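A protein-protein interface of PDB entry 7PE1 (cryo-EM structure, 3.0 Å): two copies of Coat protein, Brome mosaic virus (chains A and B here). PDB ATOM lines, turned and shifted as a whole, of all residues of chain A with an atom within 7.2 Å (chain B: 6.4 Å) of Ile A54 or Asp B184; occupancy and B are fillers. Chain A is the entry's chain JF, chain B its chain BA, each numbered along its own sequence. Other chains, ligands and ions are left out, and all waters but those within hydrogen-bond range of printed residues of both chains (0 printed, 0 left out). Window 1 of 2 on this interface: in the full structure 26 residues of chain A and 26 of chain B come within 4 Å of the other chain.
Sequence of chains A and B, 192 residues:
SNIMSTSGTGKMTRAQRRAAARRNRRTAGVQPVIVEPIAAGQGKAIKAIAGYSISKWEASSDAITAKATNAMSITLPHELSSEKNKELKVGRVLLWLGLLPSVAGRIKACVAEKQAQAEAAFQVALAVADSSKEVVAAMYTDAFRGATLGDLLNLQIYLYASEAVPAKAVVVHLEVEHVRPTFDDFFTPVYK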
ATOM      1  N   ILE A  46       1.112  -0.886   0.997  1.00  0.00           N
ATOM      2  CA  ILE A  46       1.869   0.149   1.689  1.00  0.00           C
ATOM      3  C   ILE A  46       1.314   1.516   1.317  1.00  0.00           C
ATOM      4  O   ILE A  46       0.992   1.777   0.153  1.00  0.00           O
ATOM      5  CB  ILE A  46       3.364   0.038   1.349  1.00  0.00           C
ATOM      6  CG1 ILE A  46       3.836  -1.412   1.469  1.00  0.00           C
ATOM      7  CG2 ILE A  46       4.175   0.942   2.249  1.00  0.00           C
ATOM      8  CD1 ILE A  46       3.662  -2.004   2.843  1.00  0.00           C
ATOM      9  N   LYS A  47       1.211   2.398   2.305  1.00  0.00           N
ATOM     10  CA  LYS A  47       0.635   3.724   2.124  1.00  0.00           C
ATOM     11  C   LYS A  47       1.715   4.795   2.214  1.00  0.00           C
ATOM     12  O   LYS A  47       2.577   4.752   3.096  1.00  0.00           O
ATOM     13  CB  LYS A  47      -0.453   3.986   3.167  1.00  0.00           C
ATOM     14  CG  LYS A  47      -1.173   5.302   2.985  1.00  0.00           C
ATOM     15  CD  LYS A  47      -2.227   5.499   4.051  1.00  0.00           C
ATOM     16  CE  LYS A  47      -2.911   6.840   3.894  1.00  0.00           C
ATOM     17  NZ  LYS A  47      -1.930   7.952   3.979  1.00  0.00           N
ATOM     18  N   ALA A  48       1.656   5.761   1.299  1.00  0.00           N
ATOM     19  CA  ALA A  48       2.652   6.821   1.238  1.00  0.00           C
ATOM     20  C   ALA A  48       2.534   7.757   2.436  1.00  0.00           C
ATOM     21  O   ALA A  48       1.466   7.911   3.034  1.00  0.00           O
ATOM     22  CB  ALA A  48       2.501   7.616  -0.057  1.00  0.00           C
ATOM     23  N   ILE A  49       3.652   8.392   2.784  1.00  0.00           N
ATOM     24  CA  ILE A  49       3.679   9.287   3.935  1.00  0.00           C
ATOM     25  C   ILE A  49       3.109  10.651   3.550  1.00  0.00           C
ATOM     26  O   ILE A  49       2.910  10.968   2.374  1.00  0.00           O
ATOM     27  CB  ILE A  49       5.100   9.414   4.508  1.00  0.00           C
ATOM     28  CG1 ILE A  49       5.973  10.264   3.594  1.00  0.00           C
ATOM     29  CG2 ILE A  49       5.728   8.047   4.672  1.00  0.00           C
ATOM     30  CD1 ILE A  49       7.392  10.383   4.068  1.00  0.00           C
ATOM     31  N   TYR A  52       3.318  13.243   0.124  1.00  0.00           N
ATOM     32  CA  TYR A  52       3.952  12.493  -0.948  1.00  0.00           C
ATOM     33  C   TYR A  52       2.896  11.837  -1.823  1.00  0.00           C
ATOM     34  O   TYR A  52       1.757  11.619  -1.404  1.00  0.00           O
ATOM     35  CB  TYR A  52       4.903  11.427  -0.390  1.00  0.00           C
ATOM     36  CG  TYR A  52       6.240  11.966   0.052  1.00  0.00           C
ATOM     37  CD1 TYR A  52       6.351  12.754   1.185  1.00  0.00           C
ATOM     38  CD2 TYR A  52       7.395  11.682  -0.661  1.00  0.00           C
ATOM     39  CE1 TYR A  52       7.567  13.248   1.592  1.00  0.00           C
ATOM     40  CE2 TYR A  52       8.618  12.169  -0.263  1.00  0.00           C
ATOM     41  CZ  TYR A  52       8.699  12.952   0.865  1.00  0.00           C
ATOM     42  OH  TYR A  52       9.916  13.444   1.268  1.00  0.00           O
ATOM     43  N   SER A  53       3.289  11.537  -3.058  1.00  0.00           N
ATOM     44  CA  SER A  53       2.469  10.773  -3.985  1.00  0.00           C
ATOM     45  C   SER A  53       3.359   9.767  -4.702  1.00  0.00           C
ATOM     46  O   SER A  53       4.579   9.918  -4.751  1.00  0.00           O
ATOM     47  CB  SER A  53       1.752  11.676  -4.995  1.00  0.00           C
ATOM     48  OG  SER A  53       2.671  12.365  -5.824  1.00  0.00           O
ATOM     49  N   ILE A  54       2.734   8.729  -5.249  1.00  0.00           N
ATOM     50  CA  ILE A  54       3.436   7.613  -5.877  1.00  0.00           C
ATOM     51  C   ILE A  54       3.134   7.628  -7.367  1.00  0.00           C
ATOM     52  O   ILE A  54       1.966   7.639  -7.771  1.00  0.00           O
ATOM     53  CB  ILE A  54       3.030   6.271  -5.246  1.00  0.00           C
ATOM     54  CG1 ILE A  54       3.489   6.215  -3.789  1.00  0.00           C
ATOM     55  CG2 ILE A  54       3.593   5.107  -6.042  1.00  0.00           C
ATOM     56  CD1 ILE A  54       3.028   4.996  -3.055  1.00  0.00           C
ATOM     57  N   SER A  55       4.180   7.620  -8.185  1.00  0.00           N
ATOM     58  CA  SER A  55       4.035   7.505  -9.628  1.00  0.00           C
ATOM     59  C   SER A  55       4.597   6.171 -10.106  1.00  0.00           C
ATOM     60  O   SER A  55       5.574   5.657  -9.559  1.00  0.00           O
ATOM     61  CB  SER A  55       4.733   8.659 -10.346  1.00  0.00           C
ATOM     62  OG  SER A  55       6.123   8.670 -10.081  1.00  0.00           O
ATOM     63  N   LYS A  56       3.962   5.610 -11.133  1.00  0.00           N
ATOM     64  CA  LYS A  56       4.273   4.274 -11.621  1.00  0.00           C
ATOM     65  C   LYS A  56       4.507   4.302 -13.123  1.00  0.00           C
ATOM     66  O   LYS A  56       3.812   5.013 -13.854  1.00  0.00           O
ATOM     67  CB  LYS A  56       3.136   3.292 -11.310  1.00  0.00           C
ATOM     68  CG  LYS A  56       2.613   3.348  -9.885  1.00  0.00           C
ATOM     69  CD  LYS A  56       1.428   2.413  -9.716  1.00  0.00           C
ATOM     70  CE  LYS A  56       1.060   2.201  -8.258  1.00  0.00           C
ATOM     71  NZ  LYS A  56       0.288   3.330  -7.689  1.00  0.00           N
ATOM     72  N   ARG A  92      10.622   6.266  -0.971  1.00  0.00           N
ATOM     73  CA  ARG A  92      10.912   4.854  -1.163  1.00  0.00           C
ATOM     74  C   ARG A  92      10.800   4.475  -2.634  1.00  0.00           C
ATOM     75  O   ARG A  92      10.161   5.162  -3.431  1.00  0.00           O
ATOM     76  CB  ARG A  92       9.963   3.996  -0.330  1.00  0.00           C
ATOM     77  CG  ARG A  92      10.121   4.175   1.161  1.00  0.00           C
ATOM     78  CD  ARG A  92       9.001   3.506   1.931  1.00  0.00           C
ATOM     79  NE  ARG A  92       7.752   4.251   1.852  1.00  0.00           N
ATOM     80  CZ  ARG A  92       6.645   3.928   2.506  1.00  0.00           C
ATOM     81  NH1 ARG A  92       6.599   2.877   3.306  1.00  0.00           N
ATOM     82  NH2 ARG A  92       5.560   4.679   2.354  1.00  0.00           N
ATOM     83  N   LEU A 174       8.398   0.006 -11.981  1.00  0.00           N
ATOM     84  CA  LEU A 174       9.119   0.876 -11.065  1.00  0.00           C
ATOM     85  C   LEU A 174       8.135   1.837 -10.425  1.00  0.00           C
ATOM     86  O   LEU A 174       7.364   2.496 -11.126  1.00  0.00           O
ATOM     87  CB  LEU A 174      10.218   1.643 -11.802  1.00  0.00           C
ATOM     88  CG  LEU A 174      11.427   2.116 -11.001  1.00  0.00           C
ATOM     89  CD1 LEU A 174      12.128   0.943 -10.343  1.00  0.00           C
ATOM     90  CD2 LEU A 174      12.379   2.855 -11.917  1.00  0.00           C
ATOM     91  N   GLU A 175       8.160   1.914  -9.097  1.00  0.00           N
ATOM     92  CA  GLU A 175       7.253   2.774  -8.349  1.00  0.00           C
ATOM     93  C   GLU A 175       8.073   3.675  -7.440  1.00  0.00           C
ATOM     94  O   GLU A 175       8.845   3.186  -6.611  1.00  0.00           O
ATOM     95  CB  GLU A 175       6.255   1.944  -7.547  1.00  0.00           C
ATOM     96  CG  GLU A 175       5.504   0.948  -8.404  1.00  0.00           C
ATOM     97  CD  GLU A 175       4.378   0.270  -7.665  1.00  0.00           C
ATOM     98  OE1 GLU A 175       4.062   0.706  -6.542  1.00  0.00           O
ATOM     99  OE2 GLU A 175       3.813  -0.700  -8.206  1.00  0.00           O
ATOM    100  N   VAL A 176       7.899   4.983  -7.594  1.00  0.00           N
ATOM    101  CA  VAL A 176       8.714   5.978  -6.911  1.00  0.00           C
ATOM    102  C   VAL A 176       7.798   6.858  -6.076  1.00  0.00           C
ATOM    103  O   VAL A 176       6.867   7.474  -6.605  1.00  0.00           O
ATOM    104  CB  VAL A 176       9.527   6.825  -7.901  1.00  0.00           C
ATOM    105  CG1 VAL A 176      10.366   7.841  -7.159  1.00  0.00           C
ATOM    106  CG2 VAL A 176      10.400   5.941  -8.770  1.00  0.00           C
ATOM    107  N   GLU A 177       8.070   6.926  -4.780  1.00  0.00           N
ATOM    108  CA  GLU A 177       7.390   7.853  -3.889  1.00  0.00           C
ATOM    109  C   GLU A 177       8.163   9.168  -3.869  1.00  0.00           C
ATOM    110  O   GLU A 177       9.365   9.179  -3.591  1.00  0.00           O
ATOM    111  CB  GLU A 177       7.287   7.255  -2.491  1.00  0.00           C
ATOM    112  CG  GLU A 177       6.838   8.216  -1.425  1.00  0.00           C
ATOM    113  CD  GLU A 177       6.858   7.582  -0.057  1.00  0.00           C
ATOM    114  OE1 GLU A 177       6.891   6.341   0.011  1.00  0.00           O
ATOM    115  OE2 GLU A 177       6.852   8.320   0.947  1.00  0.00           O
ATOM    116  N   HIS A 178       7.482  10.267  -4.181  1.00  0.00           N
ATOM    117  CA  HIS A 178       8.131  11.568  -4.256  1.00  0.00           C
ATOM    118  C   HIS A 178       7.161  12.638  -3.777  1.00  0.00           C
ATOM    119  O   HIS A 178       5.966  12.390  -3.610  1.00  0.00           O
ATOM    120  CB  HIS A 178       8.625  11.868  -5.675  1.00  0.00           C
ATOM    121  CG  HIS A 178       7.546  11.829  -6.709  1.00  0.00           C
ATOM    122  ND1 HIS A 178       6.705  12.893  -6.947  1.00  0.00           N
ATOM    123  CD2 HIS A 178       7.164  10.850  -7.560  1.00  0.00           C
ATOM    124  CE1 HIS A 178       5.856  12.574  -7.904  1.00  0.00           C
ATOM    125  NE2 HIS A 178       6.111  11.337  -8.292  1.00  0.00           N
ATOM    126  N   ARG A 180       4.583  15.499  -3.481  1.00  0.00           N
ATOM    127  CA  ARG A 180       3.421  15.780  -4.310  1.00  0.00           C
ATOM    128  C   ARG A 180       3.622  17.078  -5.083  1.00  0.00           C
ATOM    129  O   ARG A 180       3.954  18.107  -4.479  1.00  0.00           O
ATOM    130  CB  ARG A 180       2.178  15.875  -3.429  1.00  0.00           C
ATOM    131  CG  ARG A 180       0.951  16.393  -4.134  1.00  0.00           C
ATOM    132  CD  ARG A 180       0.078  15.258  -4.597  1.00  0.00           C
ATOM    133  NE  ARG A 180      -0.204  14.342  -3.500  1.00  0.00           N
ATOM    134  CZ  ARG A 180      -1.055  13.329  -3.571  1.00  0.00           C
ATOM    135  NH1 ARG A 180      -1.742  13.079  -4.672  1.00  0.00           N
ATOM    136  NH2 ARG A 180      -1.220  12.547  -2.507  1.00  0.00           N
ATOM    137  N   ASN B  85     -11.396   3.884 -13.946  1.00  0.00           N
ATOM    138  CA  ASN B  85     -11.238   5.328 -14.049  1.00  0.00           C
ATOM    139  C   ASN B  85     -12.236   5.987 -14.987  1.00  0.00           C
ATOM    140  O   ASN B  85     -12.444   7.199 -14.888  1.00  0.00           O
ATOM    141  CB  ASN B  85      -9.821   5.672 -14.512  1.00  0.00           C
ATOM    142  CG  ASN B  85      -8.783   5.394 -13.451  1.00  0.00           C
ATOM    143  OD1 ASN B  85      -9.045   5.537 -12.260  1.00  0.00           O
ATOM    144  ND2 ASN B  85      -7.597   4.986 -13.879  1.00  0.00           N
ATOM    145  N   ARG B 180     -11.258  13.053  -8.158  1.00  0.00           N
ATOM    146  CA  ARG B 180      -9.903  12.596  -7.891  1.00  0.00           C
ATOM    147  C   ARG B 180      -9.858  11.073  -7.836  1.00  0.00           C
ATOM    148  O   ARG B 180     -10.648  10.463  -7.104  1.00  0.00           O
ATOM    149  CB  ARG B 180      -9.417  13.189  -6.571  1.00  0.00           C
ATOM    150  CG  ARG B 180      -8.120  12.609  -6.067  1.00  0.00           C
ATOM    151  CD  ARG B 180      -6.954  13.478  -6.456  1.00  0.00           C
ATOM    152  NE  ARG B 180      -7.185  14.860  -6.059  1.00  0.00           N
ATOM    153  CZ  ARG B 180      -6.280  15.824  -6.146  1.00  0.00           C
ATOM    154  NH1 ARG B 180      -5.060  15.588  -6.597  1.00  0.00           N
ATOM    155  NH2 ARG B 180      -6.610  17.057  -5.769  1.00  0.00           N
ATOM    156  N   PRO B 181      -8.962  10.426  -8.582  1.00  0.00           N
ATOM    157  CA  PRO B 181      -8.899   8.959  -8.547  1.00  0.00           C
ATOM    158  C   PRO B 181      -8.585   8.453  -7.147  1.00  0.00           C
ATOM    159  O   PRO B 181      -7.773   9.031  -6.421  1.00  0.00           O
ATOM    160  CB  PRO B 181      -7.778   8.627  -9.538  1.00  0.00           C
ATOM    161  CG  PRO B 181      -7.679   9.825 -10.413  1.00  0.00           C
ATOM    162  CD  PRO B 181      -8.003  10.994  -9.540  1.00  0.00           C
ATOM    163  N   THR B 182      -9.231   7.343  -6.782  1.00  0.00           N
ATOM    164  CA  THR B 182      -9.306   6.948  -5.378  1.00  0.00           C
ATOM    165  C   THR B 182      -7.972   6.430  -4.853  1.00  0.00           C
ATOM    166  O   THR B 182      -7.550   6.799  -3.751  1.00  0.00           O
ATOM    167  CB  THR B 182     -10.400   5.899  -5.194  1.00  0.00           C
ATOM    168  OG1 THR B 182     -11.670   6.469  -5.536  1.00  0.00           O
ATOM    169  CG2 THR B 182     -10.438   5.405  -3.754  1.00  0.00           C
ATOM    170  N   PHE B 183      -7.291   5.580  -5.616  1.00  0.00           N
ATOM    171  CA  PHE B 183      -6.092   4.900  -5.131  1.00  0.00           C
ATOM    172  C   PHE B 183      -4.898   5.291  -5.996  1.00  0.00           C
ATOM    173  O   PHE B 183      -4.546   4.598  -6.951  1.00  0.00           O
ATOM    174  CB  PHE B 183      -6.319   3.371  -5.104  1.00  0.00           C
ATOM    175  CG  PHE B 183      -7.388   2.941  -4.141  1.00  0.00           C
ATOM    176  CD1 PHE B 183      -7.231   3.143  -2.779  1.00  0.00           C
ATOM    177  CD2 PHE B 183      -8.552   2.342  -4.592  1.00  0.00           C
ATOM    178  CE1 PHE B 183      -8.214   2.757  -1.887  1.00  0.00           C
ATOM    179  CE2 PHE B 183      -9.538   1.950  -3.702  1.00  0.00           C
ATOM    180  CZ  PHE B 183      -9.367   2.160  -2.350  1.00  0.00           C
ATOM    181  N   ASP B 184      -4.268   6.412  -5.638  1.00  0.00           N
ATOM    182  CA  ASP B 184      -2.997   6.827  -6.216  1.00  0.00           C
ATOM    183  C   ASP B 184      -1.966   7.141  -5.139  1.00  0.00           C
ATOM    184  O   ASP B 184      -0.897   7.674  -5.458  1.00  0.00           O
ATOM    185  CB  ASP B 184      -3.179   8.051  -7.126  1.00  0.00           C
ATOM    186  CG  ASP B 184      -3.799   7.699  -8.469  1.00  0.00           C
ATOM    187  OD1 ASP B 184      -3.892   6.497  -8.794  1.00  0.00           O
ATOM    188  OD2 ASP B 184      -4.197   8.630  -9.201  1.00  0.00           O
ATOM    189  N   ASP B 185      -2.266   6.834  -3.876  1.00  0.00           N
ATOM    190  CA  ASP B 185      -1.357   7.049  -2.759  1.00  0.00           C
ATOM    191  C   ASP B 185      -0.900   5.740  -2.134  1.00  0.00           C
ATOM    192  O   ASP B 185      -0.442   5.732  -0.990  1.00  0.00           O
ATOM    193  CB  ASP B 185      -2.016   7.924  -1.693  1.00  0.00           C
ATOM    194  CG  ASP B 185      -2.202   9.357  -2.143  1.00  0.00           C
ATOM    195  OD1 ASP B 185      -1.370   9.850  -2.935  1.00  0.00           O
ATOM    196  OD2 ASP B 185      -3.178   9.993  -1.696  1.00  0.00           O
ATOM    197  N   PHE B 186      -1.028   4.631  -2.855  1.00  0.00           N
ATOM    198  CA  PHE B 186      -0.735   3.318  -2.309  1.00  0.00           C
ATOM    199  C   PHE B 186       0.254   2.584  -3.198  1.00  0.00           C
ATOM    200  O   PHE B 186       0.165   2.644  -4.426  1.00  0.00           O
ATOM    201  CB  PHE B 186      -2.011   2.492  -2.152  1.00  0.00           C
ATOM    202  CG  PHE B 186      -2.836   2.884  -0.965  1.00  0.00           C
ATOM    203  CD1 PHE B 186      -2.547   2.378   0.287  1.00  0.00           C
ATOM    204  CD2 PHE B 186      -3.891   3.764  -1.097  1.00  0.00           C
ATOM    205  CE1 PHE B 186      -3.298   2.741   1.383  1.00  0.00           C
ATOM    206  CE2 PHE B 186      -4.643   4.129  -0.004  1.00  0.00           C
ATOM    207  CZ  PHE B 186      -4.346   3.616   1.237  1.00  0.00           C
ATOM    208  N   PHE B 187       1.205   1.905  -2.566  1.00  0.00           N
ATOM    209  CA  PHE B 187       2.081   0.985  -3.270  1.00  0.00           C
ATOM    210  C   PHE B 187       1.313  -0.277  -3.638  1.00  0.00           C
ATOM    211  O   PHE B 187       0.363  -0.671  -2.958  1.00  0.00           O
ATOM    212  CB  PHE B 187       3.291   0.614  -2.410  1.00  0.00           C
ATOM    213  CG  PHE B 187       4.418   1.604  -2.471  1.00  0.00           C
ATOM    214  CD1 PHE B 187       5.178   1.736  -3.617  1.00  0.00           C
ATOM    215  CD2 PHE B 187       4.739   2.377  -1.370  1.00  0.00           C
ATOM    216  CE1 PHE B 187       6.225   2.638  -3.670  1.00  0.00           C
ATOM    217  CE2 PHE B 187       5.784   3.277  -1.420  1.00  0.00           C
ATOM    218  CZ  PHE B 187       6.527   3.406  -2.570  1.00  0.00           C
ATOM    219  N   THR B 188       1.729  -0.907  -4.729  1.00  0.00           N
ATOM    220  CA  THR B 188       1.137  -2.177  -5.124  1.00  0.00           C
ATOM    221  C   THR B 188       1.536  -3.268  -4.130  1.00  0.00           C
ATOM    222  O   THR B 188       2.696  -3.329  -3.710  1.00  0.00           O
ATOM    223  CB  THR B 188       1.592  -2.548  -6.536  1.00  0.00           C
ATOM    224  OG1 THR B 188       1.145  -1.550  -7.461  1.00  0.00           O
ATOM    225  CG2 THR B 188       1.032  -3.882  -6.956  1.00  0.00           C
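The backbone carbonyl oxygen (O) of Phe B186 lies within hydrogen-bond range of the side-chain amino group (NZ) of Lys A56, 3.3 Å away. The guanidinium group (NH2) of Arg A180 lies within salt-bridge range of the side-chain carboxylate (OD1) of Asp B185, 2.7 Å away. O of Asp B185 is in hydrogen-bond range of N of Ala A48, 3.1 Å away. OE2 of Glu A175 sits at hydrogen-bond distance from OG1 of Thr B188, at 2.9 Å. The backbone NH of Phe B187 is in hydrogen-bond range of the backbone carbonyl oxygen of Ile A46, at 2.7 Å.
O of Tyr A52 is in hydrogen-bond range of NH2 of Arg A180 (3.3 Å). The guanidinium group (NE) of Arg A92 is in salt-bridge range of the side-chain carboxylate (OE1) of Glu A177, at 2.9 Å. The guanidinium group (NH2) of Arg A92 is in hydrogen-bond range of the backbone carbonyl oxygen (O) of Lys A47.
Among the printed residues, pairs that only touch across the chains: Glu A175 with Phe B187 (3.3 Å), Ile A46 with Phe B186 (3.4 Å), Ile A54 with Phe B187 (3.6 Å), Glu A177 with Phe B187 (3.6 Å), Lys A47 with Phe B186 (3.6 Å), Ile A54 with Phe B186 (3.7 Å), Ile A54 with Asp B184 (3.7 Å), Lys A56 with Thr B188 (3.8 Å), Lys A47 with Asp B185 (3.9 Å), Tyr A52 with Asp B185 (3.9 Å) and Arg A92 with Phe B187 (3.9 Å).
Printed residues of chain B within 4 Å of Tyr A52: Asp B185 (3.9 Å). Of chain B, only Asp B184 (3.7 Å), Phe B186 (3.7 Å) and Phe B187 (3.6 Å) come within 4 Å of Ile A54. Of the printed residues of chain B, Lys A56 touches Phe B186 and Thr B188. Asn B85 touches none of the printed residues of chain A. Asp B184 touches one residue of chain A. Printed residues of chain A within 4 Å of Phe B187: Ile A46, Ile A54, Arg A92, Glu A175 and Glu A177. The nearest residue of chain A that does not touch Asp B184 is Ser A53 (4.8 Å). The nearest printed residue of chain B that does not touch Arg A180 is Arg B180 (4.6 Å).
Printed residues of chain A that touch a printed residue of chain B: Ile A46, Lys A47, Ala A48, Tyr A52, Ile A54, Lys A56, Arg A92, Glu A175, Glu A177 and Arg A180. Of the 10 printed residues of chain B, 5 touch a printed residue of chain A. Among the printed residues, Asp or Glu carboxylates within 4 Å of a Lys or Arg side-chain nitrogen of the other chain: Arg A180 with Asp B185.
Position printed for both chains: 180. Of the 16 pairs that touch across the chains among the printed residues, none has its exchanged pair printed and touching as well.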
